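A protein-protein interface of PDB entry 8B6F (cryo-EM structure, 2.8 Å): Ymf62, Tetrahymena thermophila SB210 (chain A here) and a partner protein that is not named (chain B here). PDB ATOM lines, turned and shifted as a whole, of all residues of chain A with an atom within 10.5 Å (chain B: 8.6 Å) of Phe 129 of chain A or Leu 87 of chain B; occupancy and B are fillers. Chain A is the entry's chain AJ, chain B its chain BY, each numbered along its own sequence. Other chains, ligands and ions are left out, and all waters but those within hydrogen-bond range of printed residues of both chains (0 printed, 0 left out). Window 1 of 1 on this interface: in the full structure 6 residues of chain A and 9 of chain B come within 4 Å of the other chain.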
ATOM      1  N   TYR A 121      -9.396  32.324   1.992  1.00  0.00           N
ATOM      2  CA  TYR A 121      -9.474  30.910   2.342  1.00  0.00           C
ATOM      3  C   TYR A 121      -9.154  29.970   1.191  1.00  0.00           C
ATOM      4  O   TYR A 121      -8.517  28.939   1.412  1.00  0.00           O
ATOM      5  CB  TYR A 121     -10.879  30.588   2.879  1.00  0.00           C
ATOM      6  CG  TYR A 121     -11.089  29.122   3.182  1.00  0.00           C
ATOM      7  CD1 TYR A 121     -10.788  28.603   4.433  1.00  0.00           C
ATOM      8  CD2 TYR A 121     -11.587  28.256   2.217  1.00  0.00           C
ATOM      9  CE1 TYR A 121     -10.973  27.266   4.714  1.00  0.00           C
ATOM     10  CE2 TYR A 121     -11.777  26.917   2.489  1.00  0.00           C
ATOM     11  CZ  TYR A 121     -11.469  26.429   3.738  1.00  0.00           C
ATOM     12  OH  TYR A 121     -11.655  25.097   4.014  1.00  0.00           O
ATOM     13  N   TYR A 122      -9.571  30.296  -0.030  1.00  0.00           N
ATOM     14  CA  TYR A 122      -9.632  29.280  -1.072  1.00  0.00           C
ATOM     15  C   TYR A 122      -8.316  29.094  -1.817  1.00  0.00           C
ATOM     16  O   TYR A 122      -7.928  27.954  -2.095  1.00  0.00           O
ATOM     17  CB  TYR A 122     -10.753  29.614  -2.055  1.00  0.00           C
ATOM     18  CG  TYR A 122     -12.116  29.339  -1.474  1.00  0.00           C
ATOM     19  CD1 TYR A 122     -12.660  28.063  -1.503  1.00  0.00           C
ATOM     20  CD2 TYR A 122     -12.850  30.349  -0.870  1.00  0.00           C
ATOM     21  CE1 TYR A 122     -13.900  27.804  -0.961  1.00  0.00           C
ATOM     22  CE2 TYR A 122     -14.091  30.099  -0.325  1.00  0.00           C
ATOM     23  CZ  TYR A 122     -14.611  28.826  -0.375  1.00  0.00           C
ATOM     24  OH  TYR A 122     -15.849  28.581   0.169  1.00  0.00           O
ATOM     25  N   THR A 123      -7.624  30.174  -2.168  1.00  0.00           N
ATOM     26  CA  THR A 123      -6.354  30.012  -2.869  1.00  0.00           C
ATOM     27  C   THR A 123      -5.340  29.245  -2.033  1.00  0.00           C
ATOM     28  O   THR A 123      -4.764  28.268  -2.543  1.00  0.00           O
ATOM     29  CB  THR A 123      -5.807  31.379  -3.290  1.00  0.00           C
ATOM     30  OG1 THR A 123      -6.831  32.121  -3.965  1.00  0.00           O
ATOM     31  CG2 THR A 123      -4.621  31.211  -4.223  1.00  0.00           C
ATOM     32  N   PRO A 124      -5.082  29.599  -0.770  1.00  0.00           N
ATOM     33  CA  PRO A 124      -4.073  28.843  -0.010  1.00  0.00           C
ATOM     34  C   PRO A 124      -4.495  27.419   0.292  1.00  0.00           C
ATOM     35  O   PRO A 124      -3.663  26.506   0.229  1.00  0.00           O
ATOM     36  CB  PRO A 124      -3.904  29.669   1.275  1.00  0.00           C
ATOM     37  CG  PRO A 124      -4.611  30.957   1.034  1.00  0.00           C
ATOM     38  CD  PRO A 124      -5.682  30.665   0.046  1.00  0.00           C
ATOM     39  N   SER A 125      -5.770  27.202   0.615  1.00  0.00           N
ATOM     40  CA  SER A 125      -6.245  25.849   0.878  1.00  0.00           C
ATOM     41  C   SER A 125      -6.109  24.973  -0.359  1.00  0.00           C
ATOM     42  O   SER A 125      -5.699  23.810  -0.264  1.00  0.00           O
ATOM     43  CB  SER A 125      -7.695  25.882   1.358  1.00  0.00           C
ATOM     44  OG  SER A 125      -8.552  26.404   0.360  1.00  0.00           O
ATOM     45  N   LEU A 126      -6.454  25.509  -1.531  1.00  0.00           N
ATOM     46  CA  LEU A 126      -6.267  24.753  -2.764  1.00  0.00           C
ATOM     47  C   LEU A 126      -4.793  24.467  -3.016  1.00  0.00           C
ATOM     48  O   LEU A 126      -4.437  23.376  -3.474  1.00  0.00           O
ATOM     49  CB  LEU A 126      -6.865  25.507  -3.949  1.00  0.00           C
ATOM     50  CG  LEU A 126      -6.578  24.861  -5.309  1.00  0.00           C
ATOM     51  CD1 LEU A 126      -7.120  23.445  -5.366  1.00  0.00           C
ATOM     52  CD2 LEU A 126      -7.174  25.678  -6.413  1.00  0.00           C
ATOM     53  N   VAL A 127      -3.921  25.433  -2.731  1.00  0.00           N
ATOM     54  CA  VAL A 127      -2.492  25.213  -2.932  1.00  0.00           C
ATOM     55  C   VAL A 127      -2.016  24.054  -2.066  1.00  0.00           C
ATOM     56  O   VAL A 127      -1.305  23.157  -2.534  1.00  0.00           O
ATOM     57  CB  VAL A 127      -1.704  26.504  -2.645  1.00  0.00           C
ATOM     58  CG1 VAL A 127      -0.223  26.209  -2.458  1.00  0.00           C
ATOM     59  CG2 VAL A 127      -1.900  27.506  -3.771  1.00  0.00           C
ATOM     60  N   LEU A 128      -2.400  24.053  -0.789  1.00  0.00           N
ATOM     61  CA  LEU A 128      -1.989  22.969   0.097  1.00  0.00           C
ATOM     62  C   LEU A 128      -2.546  21.634  -0.375  1.00  0.00           C
ATOM     63  O   LEU A 128      -1.835  20.624  -0.387  1.00  0.00           O
ATOM     64  CB  LEU A 128      -2.438  23.256   1.529  1.00  0.00           C
ATOM     65  CG  LEU A 128      -1.753  24.419   2.244  1.00  0.00           C
ATOM     66  CD1 LEU A 128      -2.375  24.627   3.610  1.00  0.00           C
ATOM     67  CD2 LEU A 128      -0.255  24.185   2.372  1.00  0.00           C
ATOM     68  N   PHE A 129      -3.823  21.607  -0.761  1.00  0.00           N
ATOM     69  CA  PHE A 129      -4.428  20.356  -1.203  1.00  0.00           C
ATOM     70  C   PHE A 129      -3.734  19.820  -2.449  1.00  0.00           C
ATOM     71  O   PHE A 129      -3.448  18.622  -2.539  1.00  0.00           O
ATOM     72  CB  PHE A 129      -5.918  20.560  -1.468  1.00  0.00           C
ATOM     73  CG  PHE A 129      -6.629  19.312  -1.895  1.00  0.00           C
ATOM     74  CD1 PHE A 129      -7.033  18.377  -0.958  1.00  0.00           C
ATOM     75  CD2 PHE A 129      -6.894  19.074  -3.233  1.00  0.00           C
ATOM     76  CE1 PHE A 129      -7.688  17.226  -1.346  1.00  0.00           C
ATOM     77  CE2 PHE A 129      -7.549  17.925  -3.628  1.00  0.00           C
ATOM     78  CZ  PHE A 129      -7.947  16.999  -2.682  1.00  0.00           C
ATOM     79  N   LEU A 130      -3.438  20.695  -3.412  1.00  0.00           N
ATOM     80  CA  LEU A 130      -2.739  20.256  -4.616  1.00  0.00           C
ATOM     81  C   LEU A 130      -1.335  19.765  -4.293  1.00  0.00           C
ATOM     82  O   LEU A 130      -0.866  18.780  -4.874  1.00  0.00           O
ATOM     83  CB  LEU A 130      -2.683  21.389  -5.639  1.00  0.00           C
ATOM     84  CG  LEU A 130      -4.013  21.823  -6.259  1.00  0.00           C
ATOM     85  CD1 LEU A 130      -3.784  22.962  -7.233  1.00  0.00           C
ATOM     86  CD2 LEU A 130      -4.704  20.663  -6.955  1.00  0.00           C
ATOM     87  N   ILE A 131      -0.648  20.437  -3.370  1.00  0.00           N
ATOM     88  CA  ILE A 131       0.700  20.014  -3.006  1.00  0.00           C
ATOM     89  C   ILE A 131       0.681  18.606  -2.426  1.00  0.00           C
ATOM     90  O   ILE A 131       1.528  17.772  -2.765  1.00  0.00           O
ATOM     91  CB  ILE A 131       1.325  21.025  -2.023  1.00  0.00           C
ATOM     92  CG1 ILE A 131       1.646  22.347  -2.732  1.00  0.00           C
ATOM     93  CG2 ILE A 131       2.568  20.443  -1.346  1.00  0.00           C
ATOM     94  CD1 ILE A 131       2.873  22.306  -3.622  1.00  0.00           C
ATOM     95  N   PHE A 132      -0.270  18.320  -1.540  1.00  0.00           N
ATOM     96  CA  PHE A 132      -0.247  17.090  -0.761  1.00  0.00           C
ATOM     97  C   PHE A 132      -1.223  16.026  -1.249  1.00  0.00           C
ATOM     98  O   PHE A 132      -1.379  15.003  -0.577  1.00  0.00           O
ATOM     99  CB  PHE A 132      -0.535  17.406   0.705  1.00  0.00           C
ATOM    100  CG  PHE A 132       0.555  18.180   1.363  1.00  0.00           C
ATOM    101  CD1 PHE A 132       1.784  17.600   1.587  1.00  0.00           C
ATOM    102  CD2 PHE A 132       0.349  19.490   1.762  1.00  0.00           C
ATOM    103  CE1 PHE A 132       2.791  18.306   2.183  1.00  0.00           C
ATOM    104  CE2 PHE A 132       1.359  20.208   2.366  1.00  0.00           C
ATOM    105  CZ  PHE A 132       2.583  19.613   2.580  1.00  0.00           C
ATOM    106  N   PHE A 133      -1.867  16.219  -2.397  1.00  0.00           N
ATOM    107  CA  PHE A 133      -2.880  15.285  -2.874  1.00  0.00           C
ATOM    108  C   PHE A 133      -2.429  14.658  -4.183  1.00  0.00           C
ATOM    109  O   PHE A 133      -2.278  15.354  -5.192  1.00  0.00           O
ATOM    110  CB  PHE A 133      -4.229  15.980  -3.064  1.00  0.00           C
ATOM    111  CG  PHE A 133      -5.302  15.070  -3.585  1.00  0.00           C
ATOM    112  CD1 PHE A 133      -5.991  14.229  -2.730  1.00  0.00           C
ATOM    113  CD2 PHE A 133      -5.615  15.054  -4.934  1.00  0.00           C
ATOM    114  CE1 PHE A 133      -6.974  13.390  -3.211  1.00  0.00           C
ATOM    115  CE2 PHE A 133      -6.597  14.217  -5.420  1.00  0.00           C
ATOM    116  CZ  PHE A 133      -7.277  13.384  -4.557  1.00  0.00           C
ATOM    117  N   ASN A 134      -2.222  13.343  -4.160  1.00  0.00           N
ATOM    118  CA  ASN A 134      -2.068  12.566  -5.386  1.00  0.00           C
ATOM    119  C   ASN A 134      -2.375  11.118  -5.039  1.00  0.00           C
ATOM    120  O   ASN A 134      -1.622  10.493  -4.287  1.00  0.00           O
ATOM    121  CB  ASN A 134      -0.670  12.711  -5.966  1.00  0.00           C
ATOM    122  CG  ASN A 134      -0.526  12.025  -7.308  1.00  0.00           C
ATOM    123  OD1 ASN A 134      -0.020  10.906  -7.396  1.00  0.00           O
ATOM    124  ND2 ASN A 134      -0.982  12.690  -8.364  1.00  0.00           N
ATOM    125  N   ILE A 135      -3.474  10.591  -5.577  1.00  0.00           N
ATOM    126  CA  ILE A 135      -3.836   9.203  -5.319  1.00  0.00           C
ATOM    127  C   ILE A 135      -3.324   8.264  -6.403  1.00  0.00           C
ATOM    128  O   ILE A 135      -3.159   7.065  -6.142  1.00  0.00           O
ATOM    129  CB  ILE A 135      -5.359   9.048  -5.177  1.00  0.00           C
ATOM    130  CG1 ILE A 135      -5.913  10.063  -4.173  1.00  0.00           C
ATOM    131  CG2 ILE A 135      -5.694   7.640  -4.719  1.00  0.00           C
ATOM    132  CD1 ILE A 135      -7.426  10.046  -4.043  1.00  0.00           C
ATOM    133  N   LEU B  80     -18.885  25.700   4.445  1.00  0.00           N
ATOM    134  CA  LEU B  80     -17.486  26.027   4.703  1.00  0.00           C
ATOM    135  C   LEU B  80     -16.888  25.113   5.763  1.00  0.00           C
ATOM    136  O   LEU B  80     -15.727  24.703   5.651  1.00  0.00           O
ATOM    137  CB  LEU B  80     -17.354  27.491   5.125  1.00  0.00           C
ATOM    138  CG  LEU B  80     -15.922  28.002   5.311  1.00  0.00           C
ATOM    139  CD1 LEU B  80     -15.105  27.842   4.035  1.00  0.00           C
ATOM    140  CD2 LEU B  80     -15.924  29.453   5.760  1.00  0.00           C
ATOM    141  N   GLN B  81     -17.657  24.788   6.802  1.00  0.00           N
ATOM    142  CA  GLN B  81     -17.163  23.863   7.816  1.00  0.00           C
ATOM    143  C   GLN B  81     -16.940  22.474   7.233  1.00  0.00           C
ATOM    144  O   GLN B  81     -15.946  21.814   7.551  1.00  0.00           O
ATOM    145  CB  GLN B  81     -18.136  23.799   8.992  1.00  0.00           C
ATOM    146  CG  GLN B  81     -18.149  25.055   9.842  1.00  0.00           C
ATOM    147  CD  GLN B  81     -19.140  24.968  10.982  1.00  0.00           C
ATOM    148  OE1 GLN B  81     -19.685  23.904  11.266  1.00  0.00           O
ATOM    149  NE2 GLN B  81     -19.380  26.094  11.644  1.00  0.00           N
ATOM    150  N   ILE B  82     -17.858  22.006   6.386  1.00  0.00           N
ATOM    151  CA  ILE B  82     -17.679  20.696   5.765  1.00  0.00           C
ATOM    152  C   ILE B  82     -16.404  20.680   4.932  1.00  0.00           C
ATOM    153  O   ILE B  82     -15.597  19.750   5.017  1.00  0.00           O
ATOM    154  CB  ILE B  82     -18.917  20.328   4.926  1.00  0.00           C
ATOM    155  CG1 ILE B  82     -20.028  19.813   5.843  1.00  0.00           C
ATOM    156  CG2 ILE B  82     -18.573  19.288   3.857  1.00  0.00           C
ATOM    157  CD1 ILE B  82     -21.345  19.557   5.149  1.00  0.00           C
ATOM    158  N   LEU B  83     -16.205  21.714   4.111  1.00  0.00           N
ATOM    159  CA  LEU B  83     -15.013  21.759   3.269  1.00  0.00           C
ATOM    160  C   LEU B  83     -13.753  21.875   4.112  1.00  0.00           C
ATOM    161  O   LEU B  83     -12.734  21.245   3.805  1.00  0.00           O
ATOM    162  CB  LEU B  83     -15.101  22.920   2.280  1.00  0.00           C
ATOM    163  CG  LEU B  83     -13.913  23.048   1.321  1.00  0.00           C
ATOM    164  CD1 LEU B  83     -13.797  21.815   0.439  1.00  0.00           C
ATOM    165  CD2 LEU B  83     -14.030  24.300   0.471  1.00  0.00           C
ATOM    166  N   THR B  84     -13.797  22.681   5.173  1.00  0.00           N
ATOM    167  CA  THR B  84     -12.630  22.826   6.035  1.00  0.00           C
ATOM    168  C   THR B  84     -12.256  21.490   6.659  1.00  0.00           C
ATOM    169  O   THR B  84     -11.080  21.113   6.693  1.00  0.00           O
ATOM    170  CB  THR B  84     -12.904  23.870   7.119  1.00  0.00           C
ATOM    171  OG1 THR B  84     -13.284  25.110   6.511  1.00  0.00           O
ATOM    172  CG2 THR B  84     -11.668  24.094   7.975  1.00  0.00           C
ATOM    173  N   LEU B  85     -13.247  20.761   7.173  1.00  0.00           N
ATOM    174  CA  LEU B  85     -12.973  19.432   7.703  1.00  0.00           C
ATOM    175  C   LEU B  85     -12.347  18.545   6.635  1.00  0.00           C
ATOM    176  O   LEU B  85     -11.299  17.927   6.859  1.00  0.00           O
ATOM    177  CB  LEU B  85     -14.263  18.811   8.241  1.00  0.00           C
ATOM    178  CG  LEU B  85     -14.148  17.382   8.771  1.00  0.00           C
ATOM    179  CD1 LEU B  85     -13.137  17.293   9.905  1.00  0.00           C
ATOM    180  CD2 LEU B  85     -15.505  16.868   9.221  1.00  0.00           C
ATOM    181  N   ILE B  86     -12.990  18.452   5.468  1.00  0.00           N
ATOM    182  CA  ILE B  86     -12.517  17.545   4.425  1.00  0.00           C
ATOM    183  C   ILE B  86     -11.063  17.839   4.078  1.00  0.00           C
ATOM    184  O   ILE B  86     -10.226  16.932   4.014  1.00  0.00           O
ATOM    185  CB  ILE B  86     -13.418  17.646   3.179  1.00  0.00           C
ATOM    186  CG1 ILE B  86     -14.781  17.008   3.454  1.00  0.00           C
ATOM    187  CG2 ILE B  86     -12.752  16.991   1.965  1.00  0.00           C
ATOM    188  CD1 ILE B  86     -15.804  17.228   2.358  1.00  0.00           C
ATOM    189  N   LEU B  87     -10.743  19.114   3.846  1.00  0.00           N
ATOM    190  CA  LEU B  87      -9.404  19.460   3.379  1.00  0.00           C
ATOM    191  C   LEU B  87      -8.367  19.331   4.485  1.00  0.00           C
ATOM    192  O   LEU B  87      -7.291  18.760   4.273  1.00  0.00           O
ATOM    193  CB  LEU B  87      -9.402  20.880   2.808  1.00  0.00           C
ATOM    194  CG  LEU B  87     -10.138  21.083   1.481  1.00  0.00           C
ATOM    195  CD1 LEU B  87     -10.170  22.555   1.117  1.00  0.00           C
ATOM    196  CD2 LEU B  87      -9.495  20.278   0.365  1.00  0.00           C
ATOM    197  N   TYR B  88      -8.660  19.862   5.670  1.00  0.00           N
ATOM    198  CA  TYR B  88      -7.618  20.013   6.676  1.00  0.00           C
ATOM    199  C   TYR B  88      -7.442  18.796   7.567  1.00  0.00           C
ATOM    200  O   TYR B  88      -6.360  18.622   8.137  1.00  0.00           O
ATOM    201  CB  TYR B  88      -7.886  21.258   7.524  1.00  0.00           C
ATOM    202  CG  TYR B  88      -7.603  22.515   6.742  1.00  0.00           C
ATOM    203  CD1 TYR B  88      -6.303  22.974   6.586  1.00  0.00           C
ATOM    204  CD2 TYR B  88      -8.626  23.220   6.126  1.00  0.00           C
ATOM    205  CE1 TYR B  88      -6.030  24.108   5.856  1.00  0.00           C
ATOM    206  CE2 TYR B  88      -8.364  24.357   5.393  1.00  0.00           C
ATOM    207  CZ  TYR B  88      -7.063  24.797   5.263  1.00  0.00           C
ATOM    208  OH  TYR B  88      -6.795  25.931   4.535  1.00  0.00           O
ATOM    209  N   LEU B  89      -8.461  17.947   7.715  1.00  0.00           N
ATOM    210  CA  LEU B  89      -8.208  16.648   8.323  1.00  0.00           C
ATOM    211  C   LEU B  89      -7.245  15.847   7.463  1.00  0.00           C
ATOM    212  O   LEU B  89      -6.337  15.185   7.977  1.00  0.00           O
ATOM    213  CB  LEU B  89      -9.512  15.878   8.529  1.00  0.00           C
ATOM    214  CG  LEU B  89      -9.377  14.666   9.458  1.00  0.00           C
ATOM    215  CD1 LEU B  89      -9.096  15.090  10.891  1.00  0.00           C
ATOM    216  CD2 LEU B  89     -10.606  13.813   9.413  1.00  0.00           C
ATOM    217  N   PHE B  90      -7.440  15.883   6.144  1.00  0.00           N
ATOM    218  CA  PHE B  90      -6.489  15.249   5.242  1.00  0.00           C
ATOM    219  C   PHE B  90      -5.106  15.875   5.366  1.00  0.00           C
ATOM    220  O   PHE B  90      -4.095  15.165   5.399  1.00  0.00           O
ATOM    221  CB  PHE B  90      -6.992  15.349   3.802  1.00  0.00           C
ATOM    222  CG  PHE B  90      -5.942  15.054   2.776  1.00  0.00           C
ATOM    223  CD1 PHE B  90      -5.513  13.756   2.560  1.00  0.00           C
ATOM    224  CD2 PHE B  90      -5.382  16.076   2.027  1.00  0.00           C
ATOM    225  CE1 PHE B  90      -4.544  13.482   1.617  1.00  0.00           C
ATOM    226  CE2 PHE B  90      -4.414  15.808   1.083  1.00  0.00           C
ATOM    227  CZ  PHE B  90      -3.996  14.510   0.875  1.00  0.00           C
ATOM    228  N   PHE B  91      -5.042  17.206   5.437  1.00  0.00           N
ATOM    229  CA  PHE B  91      -3.754  17.879   5.552  1.00  0.00           C
ATOM    230  C   PHE B  91      -3.022  17.470   6.824  1.00  0.00           C
ATOM    231  O   PHE B  91      -1.820  17.188   6.797  1.00  0.00           O
ATOM    232  CB  PHE B  91      -3.935  19.395   5.520  1.00  0.00           C
ATOM    233  CG  PHE B  91      -2.703  20.146   5.925  1.00  0.00           C
ATOM    234  CD1 PHE B  91      -1.694  20.379   5.009  1.00  0.00           C
ATOM    235  CD2 PHE B  91      -2.541  20.597   7.224  1.00  0.00           C
ATOM    236  CE1 PHE B  91      -0.551  21.056   5.373  1.00  0.00           C
ATOM    237  CE2 PHE B  91      -1.399  21.275   7.596  1.00  0.00           C
ATOM    238  CZ  PHE B  91      -0.403  21.506   6.668  1.00  0.00           C
ATOM    239  N   ILE B  92      -3.724  17.447   7.958  1.00  0.00           N
ATOM    240  CA  ILE B  92      -3.050  17.137   9.214  1.00  0.00           C
ATOM    241  C   ILE B  92      -2.619  15.679   9.247  1.00  0.00           C
ATOM    242  O   ILE B  92      -1.549  15.346   9.769  1.00  0.00           O
ATOM    243  CB  ILE B  92      -3.958  17.494  10.407  1.00  0.00           C
ATOM    244  CG1 ILE B  92      -3.118  17.761  11.657  1.00  0.00           C
ATOM    245  CG2 ILE B  92      -4.981  16.395  10.691  1.00  0.00           C
ATOM    246  CD1 ILE B  92      -2.335  19.053  11.609  1.00  0.00           C
ATOM    247  N   THR B  93      -3.441  14.786   8.703  1.00  0.00           N
ATOM    248  CA  THR B  93      -3.062  13.381   8.651  1.00  0.00           C
ATOM    249  C   THR B  93      -1.854  13.163   7.750  1.00  0.00           C
ATOM    250  O   THR B  93      -0.960  12.377   8.081  1.00  0.00           O
ATOM    251  CB  THR B  93      -4.250  12.554   8.184  1.00  0.00           C
ATOM    252  OG1 THR B  93      -4.807  13.169   7.017  1.00  0.00           O
ATOM    253  CG2 THR B  93      -5.301  12.467   9.275  1.00  0.00           C
ATOM    254  N   ILE B  94      -1.808  13.843   6.601  1.00  0.00           N
ATOM    255  CA  ILE B  94      -0.656  13.697   5.718  1.00  0.00           C
ATOM    256  C   ILE B  94       0.575  14.317   6.359  1.00  0.00           C
ATOM    257  O   ILE B  94       1.693  13.821   6.183  1.00  0.00           O
ATOM    258  CB  ILE B  94      -0.955  14.300   4.329  1.00  0.00           C
ATOM    259  CG1 ILE B  94      -0.290  13.469   3.228  1.00  0.00           C
ATOM    260  CG2 ILE B  94      -0.468  15.740   4.216  1.00  0.00           C
ATOM    261  CD1 ILE B  94      -0.911  12.109   3.012  1.00  0.00           C
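The side-chain hydroxyl of Thr 84 of chain B is in hydrogen-bond range of the side-chain hydroxyl of Tyr 121 of chain A (3.0 Å).
The side-chain hydroxyl (OG1) of Thr 93 of chain B sits at hydrogen-bond distance from the backbone carbonyl oxygen (O) of Phe 90 of chain B (2.7 Å). The backbone carbonyl oxygen (O) of Tyr 121 of chain A is in hydrogen-bond range of the side-chain hydroxyl (OG) of Ser 125 of chain A (2.7 Å). The backbone carbonyl oxygen of Leu 80 of chain B is in hydrogen-bond range of the side-chain hydroxyl of Thr 84 of chain B (2.6 Å). The backbone carbonyl oxygen (O) of Tyr 122 of chain A lies within hydrogen-bond range of the side-chain hydroxyl (OG) of Ser 125 of chain A.
Leu 80 of chain B touches Tyr 121 of chain A. Tyr 121 of chain A touches Leu 83 of chain B (OH to C, 3.8 Å). Tyr 121 of chain A touches Tyr 88 of chain B. Tyr 122 of chain A touches Leu 83 of chain B (CE1 to CD2, 3.8 Å). Tyr 88 of chain B touches Ser 125 of chain A (OH to CB, 3.3 Å). CD1 of Phe 129 of chain A touches CD2 of Leu 87 of chain B, at 3.4 Å. CZ of Phe 90 of chain B touches O of Phe 132 of chain A, 3.0 Å away. CE2 of Phe 132 of chain A touches CE1 of Phe 91 of chain B, at 3.7 Å. CB of Phe 132 of chain A touches CG2 of Ile 94 of chain B, at 3.9 Å. Phe 133 of chain A touches Phe 90 of chain B (CA to CZ, 3.99 Å).
Of the printed residues of chain B, Tyr 121 of chain A touches Leu 80, Leu 83, Thr 84 and Tyr 88. Printed residues of chain B within 4 Å of Ser 125 of chain A: Tyr 88. Phe 129 of chain A touches just one residue of chain B: Leu 87. Of the printed residues of chain B, Phe 132 of chain A touches Phe 90, Phe 91 and Ile 94. Leu 83 of chain B touches two residues of chain A. No residue of chain A comes within 4 Å of Ile 86 of chain B. Leu 87 of chain B touches just one residue of chain A: Phe 129 (3.4 Å). Of the printed residues of chain A, Tyr 88 of chain B touches Tyr 121 (3.6 Å) and Ser 125 (3.3 Å). Printed residues of chain A within 4 Å of Ile 94 of chain B: Phe 132 (3.9 Å). The nearest residue of chain B that does not touch Phe 129 of chain A is Phe 90 of chain B (4.1 Å). The nearest printed residue of chain A that does not touch Leu 87 of chain B is Tyr 121 of chain A (4.1 Å).
Of the 15 printed residues of chain A, 6 touch a printed residue of chain B. Printed residues of chain A that touch a printed residue of chain B: Tyr 121, Tyr 122, Ser 125, Phe 129, Phe 132 and Phe 133. Hydrophobic or aromatic side chains of chain A within 4 Å of the printed part of chain B: Tyr 121, Tyr 122, Phe 129 and Phe 132. Of the 15 printed residues of chain B, 8 touch a printed residue of chain A.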
